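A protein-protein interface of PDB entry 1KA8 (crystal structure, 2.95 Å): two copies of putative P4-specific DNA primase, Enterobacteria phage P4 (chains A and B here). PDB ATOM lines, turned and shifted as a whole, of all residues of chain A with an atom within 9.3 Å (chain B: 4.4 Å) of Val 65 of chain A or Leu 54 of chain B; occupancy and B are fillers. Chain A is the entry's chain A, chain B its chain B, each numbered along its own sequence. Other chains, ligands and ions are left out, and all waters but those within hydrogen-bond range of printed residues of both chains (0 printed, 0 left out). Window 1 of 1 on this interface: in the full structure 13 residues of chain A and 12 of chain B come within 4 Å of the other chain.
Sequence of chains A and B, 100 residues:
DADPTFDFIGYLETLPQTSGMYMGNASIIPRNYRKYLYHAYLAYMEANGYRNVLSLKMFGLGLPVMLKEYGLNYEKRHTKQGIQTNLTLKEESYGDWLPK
Of the printed residues of chain B, Pro 64 of chain A touches Met 58.
Printed residues of chain A within 4 Å of Thr 5 of chain B: Glu 69.
Of chain A, only Val 65 (3.8 Å) and Glu 69 (3.96 Å) come within 4 Å of Leu 54 of chain B.
Of the printed residues of chain A, Met 58 of chain B touches Pro 64 (3.7 Å) and Val 65 (3.0 Å).
Of the printed residues of chain A, Leu 61 of chain B touches Val 65 (3.7 Å).
Positions printed for both chains: 5, 58, 59, 61 and 62.
Of the 7 pairs that touch across the chains among the printed residues, none has its exchanged pair printed and touching as well.
Of the 20 printed residues of chain A, 3 touch a printed residue of chain B.
Hydrophobic or aromatic side chains of chain A that line the printed part of chain B: Val 65.
Of the 11 printed residues of chain B, 5 touch a printed residue of chain A.
Among the printed residues, 7 pairs touch across the chains.
The side-chain hydroxyl of Thr 5 of chain B is in hydrogen-bond range of the side-chain hydroxyl of Tyr 41 of chain B.
The backbone carbonyl oxygen (O) of Leu 54 of chain B sits at hydrogen-bond distance from the side-chain hydroxyl (OH) of Tyr 38 of chain B (2.5 Å).
The side-chain hydroxyl (OH) of Tyr 41 of chain B is in hydrogen-bond range of the backbone NH (N) of Leu 54 of chain B (3.2 Å).
The side-chain hydroxyl (OG) of Ser 55 of chain B sits at hydrogen-bond distance from the backbone NH (N) of Met 58 of chain B.
Met 58 of chain B touches Pro 64 of chain A (CE to C, 3.7 Å).
Val 65 of chain A touches Leu 54 of chain B.
Met 58 of chain B touches Val 65 of chain A.
CB of Leu 61 of chain B touches CG2 of Val 65 of chain A (3.7 Å).
Gly 62 of chain B touches Val 65 of chain A.
Glu 69 of chain A touches Thr 5 of chain B.
CG of Glu 69 of chain A touches CD2 of Leu 54 of chain B, at 3.96 Å.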
ATOM      1  N   THR A   5     -29.160 -23.300  17.713  1.00  0.00           N
ATOM      2  CA  THR A   5     -29.228 -21.892  18.056  1.00  0.00           C
ATOM      3  C   THR A   5     -28.607 -21.061  16.931  1.00  0.00           C
ATOM      4  O   THR A   5     -29.146 -20.028  16.522  1.00  0.00           O
ATOM      5  CB  THR A   5     -28.467 -21.613  19.358  1.00  0.00           C
ATOM      6  OG1 THR A   5     -29.225 -22.110  20.475  1.00  0.00           O
ATOM      7  CG2 THR A   5     -28.194 -20.123  19.504  1.00  0.00           C
ATOM      8  N   PHE A   6     -27.471 -21.522  16.427  1.00  0.00           N
ATOM      9  CA  PHE A   6     -26.787 -20.826  15.344  1.00  0.00           C
ATOM     10  C   PHE A   6     -27.615 -20.779  14.056  1.00  0.00           C
ATOM     11  O   PHE A   6     -27.674 -19.741  13.383  1.00  0.00           O
ATOM     12  CB  PHE A   6     -25.480 -21.510  15.019  1.00  0.00           C
ATOM     13  CG  PHE A   6     -24.744 -20.871  13.906  1.00  0.00           C
ATOM     14  CD1 PHE A   6     -23.996 -19.712  14.133  1.00  0.00           C
ATOM     15  CD2 PHE A   6     -24.821 -21.401  12.624  1.00  0.00           C
ATOM     16  CE1 PHE A   6     -23.313 -19.062  13.071  1.00  0.00           C
ATOM     17  CE2 PHE A   6     -24.153 -20.777  11.554  1.00  0.00           C
ATOM     18  CZ  PHE A   6     -23.392 -19.598  11.771  1.00  0.00           C
ATOM     19  N   ILE A   9     -30.350 -18.222  14.189  1.00  0.00           N
ATOM     20  CA  ILE A   9     -29.822 -16.882  13.946  1.00  0.00           C
ATOM     21  C   ILE A   9     -29.626 -16.634  12.449  1.00  0.00           C
ATOM     22  O   ILE A   9     -29.405 -15.504  12.000  1.00  0.00           O
ATOM     23  CB  ILE A   9     -28.486 -16.693  14.687  1.00  0.00           C
ATOM     24  CG1 ILE A   9     -28.641 -17.118  16.149  1.00  0.00           C
ATOM     25  CG2 ILE A   9     -28.032 -15.255  14.600  1.00  0.00           C
ATOM     26  CD1 ILE A   9     -29.794 -16.492  16.859  1.00  0.00           C
ATOM     27  N   MET A  58     -28.741 -17.221  28.617  1.00  0.00           N
ATOM     28  CA  MET A  58     -27.728 -17.812  27.752  1.00  0.00           C
ATOM     29  C   MET A  58     -27.930 -17.356  26.329  1.00  0.00           C
ATOM     30  O   MET A  58     -26.981 -16.962  25.652  1.00  0.00           O
ATOM     31  CB  MET A  58     -27.754 -19.351  27.852  1.00  0.00           C
ATOM     32  CG  MET A  58     -27.138 -19.894  29.170  1.00  0.00           C
ATOM     33  SD  MET A  58     -25.443 -19.229  29.485  1.00  0.00           S
ATOM     34  CE  MET A  58     -24.436 -20.547  28.722  1.00  0.00           C
ATOM     35  N   PHE A  59     -29.178 -17.394  25.887  1.00  0.00           N
ATOM     36  CA  PHE A  59     -29.524 -16.966  24.543  1.00  0.00           C
ATOM     37  C   PHE A  59     -29.026 -15.533  24.364  1.00  0.00           C
ATOM     38  O   PHE A  59     -28.350 -15.186  23.392  1.00  0.00           O
ATOM     39  CB  PHE A  59     -31.036 -17.000  24.374  1.00  0.00           C
ATOM     40  CG  PHE A  59     -31.492 -16.634  23.002  1.00  0.00           C
ATOM     41  CD1 PHE A  59     -31.690 -17.623  22.037  1.00  0.00           C
ATOM     42  CD2 PHE A  59     -31.704 -15.298  22.661  1.00  0.00           C
ATOM     43  CE1 PHE A  59     -32.093 -17.293  20.750  1.00  0.00           C
ATOM     44  CE2 PHE A  59     -32.107 -14.950  21.376  1.00  0.00           C
ATOM     45  CZ  PHE A  59     -32.304 -15.952  20.414  1.00  0.00           C
ATOM     46  N   GLY A  60     -29.361 -14.702  25.335  1.00  0.00           N
ATOM     47  CA  GLY A  60     -28.960 -13.317  25.275  1.00  0.00           C
ATOM     48  C   GLY A  60     -27.484 -13.153  24.986  1.00  0.00           C
ATOM     49  O   GLY A  60     -27.102 -12.435  24.070  1.00  0.00           O
ATOM     50  N   LEU A  61     -26.655 -13.814  25.782  1.00  0.00           N
ATOM     51  CA  LEU A  61     -25.197 -13.766  25.637  1.00  0.00           C
ATOM     52  C   LEU A  61     -24.709 -14.168  24.256  1.00  0.00           C
ATOM     53  O   LEU A  61     -23.843 -13.521  23.660  1.00  0.00           O
ATOM     54  CB  LEU A  61     -24.529 -14.741  26.601  1.00  0.00           C
ATOM     55  CG  LEU A  61     -24.435 -14.477  28.096  1.00  0.00           C
ATOM     56  CD1 LEU A  61     -23.609 -15.609  28.732  1.00  0.00           C
ATOM     57  CD2 LEU A  61     -23.774 -13.120  28.342  1.00  0.00           C
ATOM     58  N   GLY A  62     -25.244 -15.283  23.773  1.00  0.00           N
ATOM     59  CA  GLY A  62     -24.830 -15.796  22.487  1.00  0.00           C
ATOM     60  C   GLY A  62     -25.212 -14.929  21.322  1.00  0.00           C
ATOM     61  O   GLY A  62     -24.404 -14.740  20.407  1.00  0.00           O
ATOM     62  N   LEU A  63     -26.441 -14.400  21.359  1.00  0.00           N
ATOM     63  CA  LEU A  63     -26.982 -13.544  20.295  1.00  0.00           C
ATOM     64  C   LEU A  63     -25.927 -12.655  19.614  1.00  0.00           C
ATOM     65  O   LEU A  63     -25.606 -12.865  18.443  1.00  0.00           O
ATOM     66  CB  LEU A  63     -28.105 -12.669  20.854  1.00  0.00           C
ATOM     67  CG  LEU A  63     -29.306 -12.310  19.976  1.00  0.00           C
ATOM     68  CD1 LEU A  63     -30.024 -11.151  20.635  1.00  0.00           C
ATOM     69  CD2 LEU A  63     -28.873 -11.938  18.565  1.00  0.00           C
ATOM     70  N   PRO A  64     -25.365 -11.668  20.342  1.00  0.00           N
ATOM     71  CA  PRO A  64     -24.354 -10.764  19.787  1.00  0.00           C
ATOM     72  C   PRO A  64     -23.258 -11.478  19.025  1.00  0.00           C
ATOM     73  O   PRO A  64     -22.878 -11.081  17.924  1.00  0.00           O
ATOM     74  CB  PRO A  64     -23.793 -10.079  21.027  1.00  0.00           C
ATOM     75  CG  PRO A  64     -24.941 -10.038  21.927  1.00  0.00           C
ATOM     76  CD  PRO A  64     -25.513 -11.420  21.783  1.00  0.00           C
ATOM     77  N   VAL A  65     -22.745 -12.531  19.640  1.00  0.00           N
ATOM     78  CA  VAL A  65     -21.671 -13.327  19.065  1.00  0.00           C
ATOM     79  C   VAL A  65     -22.055 -13.974  17.737  1.00  0.00           C
ATOM     80  O   VAL A  65     -21.433 -13.703  16.706  1.00  0.00           O
ATOM     81  CB  VAL A  65     -21.230 -14.445  20.066  1.00  0.00           C
ATOM     82  CG1 VAL A  65     -20.007 -15.184  19.544  1.00  0.00           C
ATOM     83  CG2 VAL A  65     -20.939 -13.838  21.439  1.00  0.00           C
ATOM     84  N   MET A  66     -23.077 -14.824  17.766  1.00  0.00           N
ATOM     85  CA  MET A  66     -23.521 -15.518  16.563  1.00  0.00           C
ATOM     86  C   MET A  66     -23.911 -14.568  15.428  1.00  0.00           C
ATOM     87  O   MET A  66     -23.720 -14.886  14.252  1.00  0.00           O
ATOM     88  CB  MET A  66     -24.680 -16.446  16.908  1.00  0.00           C
ATOM     89  CG  MET A  66     -24.413 -17.322  18.123  1.00  0.00           C
ATOM     90  SD  MET A  66     -25.538 -18.725  18.148  1.00  0.00           S
ATOM     91  CE  MET A  66     -24.886 -19.709  19.518  1.00  0.00           C
ATOM     92  N   LEU A  67     -24.462 -13.407  15.778  1.00  0.00           N
ATOM     93  CA  LEU A  67     -24.831 -12.415  14.767  1.00  0.00           C
ATOM     94  C   LEU A  67     -23.561 -11.949  14.069  1.00  0.00           C
ATOM     95  O   LEU A  67     -23.509 -11.869  12.842  1.00  0.00           O
ATOM     96  CB  LEU A  67     -25.525 -11.198  15.402  1.00  0.00           C
ATOM     97  CG  LEU A  67     -27.002 -11.315  15.803  1.00  0.00           C
ATOM     98  CD1 LEU A  67     -27.425 -10.030  16.486  1.00  0.00           C
ATOM     99  CD2 LEU A  67     -27.872 -11.590  14.583  1.00  0.00           C
ATOM    100  N   LYS A  68     -22.540 -11.631  14.866  1.00  0.00           N
ATOM    101  CA  LYS A  68     -21.253 -11.185  14.332  1.00  0.00           C
ATOM    102  C   LYS A  68     -20.725 -12.248  13.381  1.00  0.00           C
ATOM    103  O   LYS A  68     -20.152 -11.936  12.331  1.00  0.00           O
ATOM    104  CB  LYS A  68     -20.214 -10.991  15.449  1.00  0.00           C
ATOM    105  CG  LYS A  68     -19.601  -9.577  15.521  1.00  0.00           C
ATOM    106  CD  LYS A  68     -19.279  -8.964  14.125  1.00  0.00           C
ATOM    107  CE  LYS A  68     -18.943  -7.441  14.212  1.00  0.00           C
ATOM    108  NZ  LYS A  68     -18.995  -6.661  12.912  1.00  0.00           N
ATOM    109  N   GLU A  69     -20.913 -13.508  13.770  1.00  0.00           N
ATOM    110  CA  GLU A  69     -20.467 -14.625  12.954  1.00  0.00           C
ATOM    111  C   GLU A  69     -21.142 -14.595  11.589  1.00  0.00           C
ATOM    112  O   GLU A  69     -20.564 -15.016  10.584  1.00  0.00           O
ATOM    113  CB  GLU A  69     -20.762 -15.954  13.646  1.00  0.00           C
ATOM    114  CG  GLU A  69     -19.787 -16.297  14.748  1.00  0.00           C
ATOM    115  CD  GLU A  69     -19.875 -17.750  15.115  1.00  0.00           C
ATOM    116  OE1 GLU A  69     -18.843 -18.455  15.009  1.00  0.00           O
ATOM    117  OE2 GLU A  69     -20.985 -18.190  15.493  1.00  0.00           O
ATOM    118  N   TYR A  70     -22.372 -14.098  11.554  1.00  0.00           N
ATOM    119  CA  TYR A  70     -23.109 -13.987  10.297  1.00  0.00           C
ATOM    120  C   TYR A  70     -22.806 -12.633   9.655  1.00  0.00           C
ATOM    121  O   TYR A  70     -23.325 -12.312   8.596  1.00  0.00           O
ATOM    122  CB  TYR A  70     -24.616 -14.113  10.550  1.00  0.00           C
ATOM    123  CG  TYR A  70     -25.132 -15.539  10.691  1.00  0.00           C
ATOM    124  CD1 TYR A  70     -25.529 -16.052  11.942  1.00  0.00           C
ATOM    125  CD2 TYR A  70     -25.341 -16.335   9.556  1.00  0.00           C
ATOM    126  CE1 TYR A  70     -26.140 -17.309  12.046  1.00  0.00           C
ATOM    127  CE2 TYR A  70     -25.950 -17.588   9.652  1.00  0.00           C
ATOM    128  CZ  TYR A  70     -26.353 -18.065  10.892  1.00  0.00           C
ATOM    129  OH  TYR A  70     -27.023 -19.274  10.950  1.00  0.00           O
ATOM    130  N   GLY A  71     -21.969 -11.843  10.314  1.00  0.00           N
ATOM    131  CA  GLY A  71     -21.614 -10.540   9.788  1.00  0.00           C
ATOM    132  C   GLY A  71     -22.666  -9.467   9.983  1.00  0.00           C
ATOM    133  O   GLY A  71     -22.780  -8.552   9.180  1.00  0.00           O
ATOM    134  N   LEU A  72     -23.438  -9.570  11.053  1.00  0.00           N
ATOM    135  CA  LEU A  72     -24.478  -8.588  11.331  1.00  0.00           C
ATOM    136  C   LEU A  72     -24.164  -7.828  12.613  1.00  0.00           C
ATOM    137  O   LEU A  72     -23.458  -8.332  13.494  1.00  0.00           O
ATOM    138  CB  LEU A  72     -25.834  -9.278  11.479  1.00  0.00           C
ATOM    139  CG  LEU A  72     -26.088 -10.346  10.421  1.00  0.00           C
ATOM    140  CD1 LEU A  72     -27.443 -10.988  10.609  1.00  0.00           C
ATOM    141  CD2 LEU A  72     -25.972  -9.706   9.065  1.00  0.00           C
ATOM    142  N   ASN A  73     -24.708  -6.620  12.715  1.00  0.00           N
ATOM    143  CA  ASN A  73     -24.510  -5.745  13.874  1.00  0.00           C
ATOM    144  C   ASN A  73     -25.695  -5.727  14.836  1.00  0.00           C
ATOM    145  O   ASN A  73     -26.684  -5.030  14.582  1.00  0.00           O
ATOM    146  CB  ASN A  73     -24.341  -4.290  13.437  1.00  0.00           C
ATOM    147  CG  ASN A  73     -22.960  -3.965  12.968  1.00  0.00           C
ATOM    148  OD1 ASN A  73     -22.639  -2.787  12.793  1.00  0.00           O
ATOM    149  ND2 ASN A  73     -22.127  -4.992  12.753  1.00  0.00           N
ATOM    150  N   TYR A  74     -25.588  -6.441  15.952  1.00  0.00           N
ATOM    151  CA  TYR A  74     -26.665  -6.465  16.932  1.00  0.00           C
ATOM    152  C   TYR A  74     -26.826  -5.092  17.571  1.00  0.00           C
ATOM    153  O   TYR A  74     -25.842  -4.394  17.810  1.00  0.00           O
ATOM    154  CB  TYR A  74     -26.362  -7.509  18.003  1.00  0.00           C
ATOM    155  CG  TYR A  74     -27.362  -7.569  19.126  1.00  0.00           C
ATOM    156  CD1 TYR A  74     -28.666  -8.016  18.911  1.00  0.00           C
ATOM    157  CD2 TYR A  74     -26.992  -7.203  20.419  1.00  0.00           C
ATOM    158  CE1 TYR A  74     -29.569  -8.101  19.962  1.00  0.00           C
ATOM    159  CE2 TYR A  74     -27.887  -7.285  21.476  1.00  0.00           C
ATOM    160  CZ  TYR A  74     -29.169  -7.737  21.242  1.00  0.00           C
ATOM    161  OH  TYR A  74     -30.028  -7.847  22.301  1.00  0.00           O
ATOM    162  N   THR B   5     -16.257 -21.998  14.963  1.00  0.00           N
ATOM    163  CA  THR B   5     -16.045 -21.843  16.377  1.00  0.00           C
ATOM    164  C   THR B   5     -16.791 -22.918  17.136  1.00  0.00           C
ATOM    165  O   THR B   5     -16.273 -23.487  18.101  1.00  0.00           O
ATOM    166  CB  THR B   5     -16.489 -20.492  16.846  1.00  0.00           C
ATOM    167  OG1 THR B   5     -15.431 -19.565  16.598  1.00  0.00           O
ATOM    168  CG2 THR B   5     -16.786 -20.505  18.330  1.00  0.00           C
ATOM    169  N   TYR B  38      -7.465 -19.857  23.951  1.00  0.00           N
ATOM    170  CA  TYR B  38      -7.565 -18.961  22.816  1.00  0.00           C
ATOM    171  C   TYR B  38      -6.579 -19.339  21.711  1.00  0.00           C
ATOM    172  O   TYR B  38      -6.932 -19.329  20.523  1.00  0.00           O
ATOM    173  CB  TYR B  38      -7.326 -17.519  23.259  1.00  0.00           C
ATOM    174  CG  TYR B  38      -7.831 -16.568  22.220  1.00  0.00           C
ATOM    175  CD1 TYR B  38      -9.168 -16.591  21.848  1.00  0.00           C
ATOM    176  CD2 TYR B  38      -6.962 -15.714  21.529  1.00  0.00           C
ATOM    177  CE1 TYR B  38      -9.633 -15.804  20.816  1.00  0.00           C
ATOM    178  CE2 TYR B  38      -7.419 -14.916  20.482  1.00  0.00           C
ATOM    179  CZ  TYR B  38      -8.759 -14.975  20.134  1.00  0.00           C
ATOM    180  OH  TYR B  38      -9.244 -14.241  19.083  1.00  0.00           O
ATOM    181  N   TYR B  41      -7.696 -22.243  19.901  1.00  0.00           N
ATOM    182  CA  TYR B  41      -8.736 -21.745  18.991  1.00  0.00           C
ATOM    183  C   TYR B  41      -8.122 -21.244  17.653  1.00  0.00           C
ATOM    184  O   TYR B  41      -8.489 -21.704  16.557  1.00  0.00           O
ATOM    185  CB  TYR B  41      -9.510 -20.622  19.702  1.00  0.00           C
ATOM    186  CG  TYR B  41     -10.590 -19.977  18.880  1.00  0.00           C
ATOM    187  CD1 TYR B  41     -11.527 -20.748  18.191  1.00  0.00           C
ATOM    188  CD2 TYR B  41     -10.659 -18.591  18.761  1.00  0.00           C
ATOM    189  CE1 TYR B  41     -12.503 -20.148  17.396  1.00  0.00           C
ATOM    190  CE2 TYR B  41     -11.626 -17.979  17.970  1.00  0.00           C
ATOM    191  CZ  TYR B  41     -12.540 -18.764  17.291  1.00  0.00           C
ATOM    192  OH  TYR B  41     -13.481 -18.160  16.494  1.00  0.00           O
ATOM    193  N   VAL B  53     -11.179 -14.754  12.559  1.00  0.00           N
ATOM    194  CA  VAL B  53     -11.521 -15.463  13.786  1.00  0.00           C
ATOM    195  C   VAL B  53     -12.124 -14.537  14.837  1.00  0.00           C
ATOM    196  O   VAL B  53     -11.852 -13.335  14.843  1.00  0.00           O
ATOM    197  CB  VAL B  53     -10.282 -16.136  14.363  1.00  0.00           C
ATOM    198  CG1 VAL B  53      -9.551 -16.882  13.252  1.00  0.00           C
ATOM    199  CG2 VAL B  53      -9.381 -15.098  15.014  1.00  0.00           C
ATOM    200  N   LEU B  54     -12.954 -15.091  15.720  1.00  0.00           N
ATOM    201  CA  LEU B  54     -13.552 -14.288  16.784  1.00  0.00           C
ATOM    202  C   LEU B  54     -12.469 -13.687  17.680  1.00  0.00           C
ATOM    203  O   LEU B  54     -11.437 -14.306  17.939  1.00  0.00           O
ATOM    204  CB  LEU B  54     -14.481 -15.120  17.664  1.00  0.00           C
ATOM    205  CG  LEU B  54     -15.724 -15.759  17.066  1.00  0.00           C
ATOM    206  CD1 LEU B  54     -16.611 -16.278  18.194  1.00  0.00           C
ATOM    207  CD2 LEU B  54     -16.483 -14.743  16.269  1.00  0.00           C
ATOM    208  N   SER B  55     -12.707 -12.476  18.152  1.00  0.00           N
ATOM    209  CA  SER B  55     -11.753 -11.823  19.027  1.00  0.00           C
ATOM    210  C   SER B  55     -11.822 -12.543  20.365  1.00  0.00           C
ATOM    211  O   SER B  55     -12.727 -13.342  20.614  1.00  0.00           O
ATOM    212  CB  SER B  55     -12.122 -10.355  19.237  1.00  0.00           C
ATOM    213  OG  SER B  55     -13.247 -10.216  20.096  1.00  0.00           O
ATOM    214  N   LEU B  56     -10.860 -12.259  21.225  1.00  0.00           N
ATOM    215  CA  LEU B  56     -10.842 -12.869  22.531  1.00  0.00           C
ATOM    216  C   LEU B  56     -12.153 -12.540  23.201  1.00  0.00           C
ATOM    217  O   LEU B  56     -12.833 -13.430  23.692  1.00  0.00           O
ATOM    218  CB  LEU B  56      -9.686 -12.317  23.358  1.00  0.00           C
ATOM    219  CG  LEU B  56      -9.764 -12.466  24.875  1.00  0.00           C
ATOM    220  CD1 LEU B  56      -9.828 -13.927  25.259  1.00  0.00           C
ATOM    221  CD2 LEU B  56      -8.545 -11.810  25.498  1.00  0.00           C
ATOM    222  N   MET B  58     -15.130 -11.641  21.983  1.00  0.00           N
ATOM    223  CA  MET B  58     -16.269 -12.332  21.406  1.00  0.00           C
ATOM    224  C   MET B  58     -16.182 -13.838  21.702  1.00  0.00           C
ATOM    225  O   MET B  58     -17.176 -14.465  22.090  1.00  0.00           O
ATOM    226  CB  MET B  58     -16.369 -12.059  19.895  1.00  0.00           C
ATOM    227  CG  MET B  58     -16.895 -10.653  19.557  1.00  0.00           C
ATOM    228  SD  MET B  58     -18.375 -10.125  20.534  1.00  0.00           S
ATOM    229  CE  MET B  58     -19.662 -11.143  19.758  1.00  0.00           C
ATOM    230  N   PHE B  59     -14.992 -14.414  21.541  1.00  0.00           N
ATOM    231  CA  PHE B  59     -14.801 -15.832  21.815  1.00  0.00           C
ATOM    232  C   PHE B  59     -15.218 -16.117  23.252  1.00  0.00           C
ATOM    233  O   PHE B  59     -15.937 -17.083  23.548  1.00  0.00           O
ATOM    234  CB  PHE B  59     -13.332 -16.223  21.630  1.00  0.00           C
ATOM    235  CG  PHE B  59     -13.053 -17.663  21.970  1.00  0.00           C
ATOM    236  CD1 PHE B  59     -13.484 -18.689  21.125  1.00  0.00           C
ATOM    237  CD2 PHE B  59     -12.434 -18.004  23.175  1.00  0.00           C
ATOM    238  CE1 PHE B  59     -13.309 -20.025  21.480  1.00  0.00           C
ATOM    239  CE2 PHE B  59     -12.259 -19.335  23.533  1.00  0.00           C
ATOM    240  CZ  PHE B  59     -12.700 -20.347  22.680  1.00  0.00           C
ATOM    241  N   LEU B  61     -17.310 -14.586  25.263  1.00  0.00           N
ATOM    242  CA  LEU B  61     -18.762 -14.562  25.448  1.00  0.00           C
ATOM    243  C   LEU B  61     -19.444 -15.802  24.906  1.00  0.00           C
ATOM    244  O   LEU B  61     -20.331 -16.361  25.552  1.00  0.00           O
ATOM    245  CB  LEU B  61     -19.352 -13.320  24.776  1.00  0.00           C
ATOM    246  CG  LEU B  61     -18.912 -12.017  25.448  1.00  0.00           C
ATOM    247  CD1 LEU B  61     -19.062 -10.826  24.506  1.00  0.00           C
ATOM    248  CD2 LEU B  61     -19.727 -11.846  26.720  1.00  0.00           C
ATOM    249  N   GLY B  62     -19.022 -16.233  23.722  1.00  0.00           N
ATOM    250  CA  GLY B  62     -19.615 -17.405  23.109  1.00  0.00           C
ATOM    251  C   GLY B  62     -19.334 -18.690  23.852  1.00  0.00           C
ATOM    252  O   GLY B  62     -20.247 -19.518  24.018  1.00  0.00           O
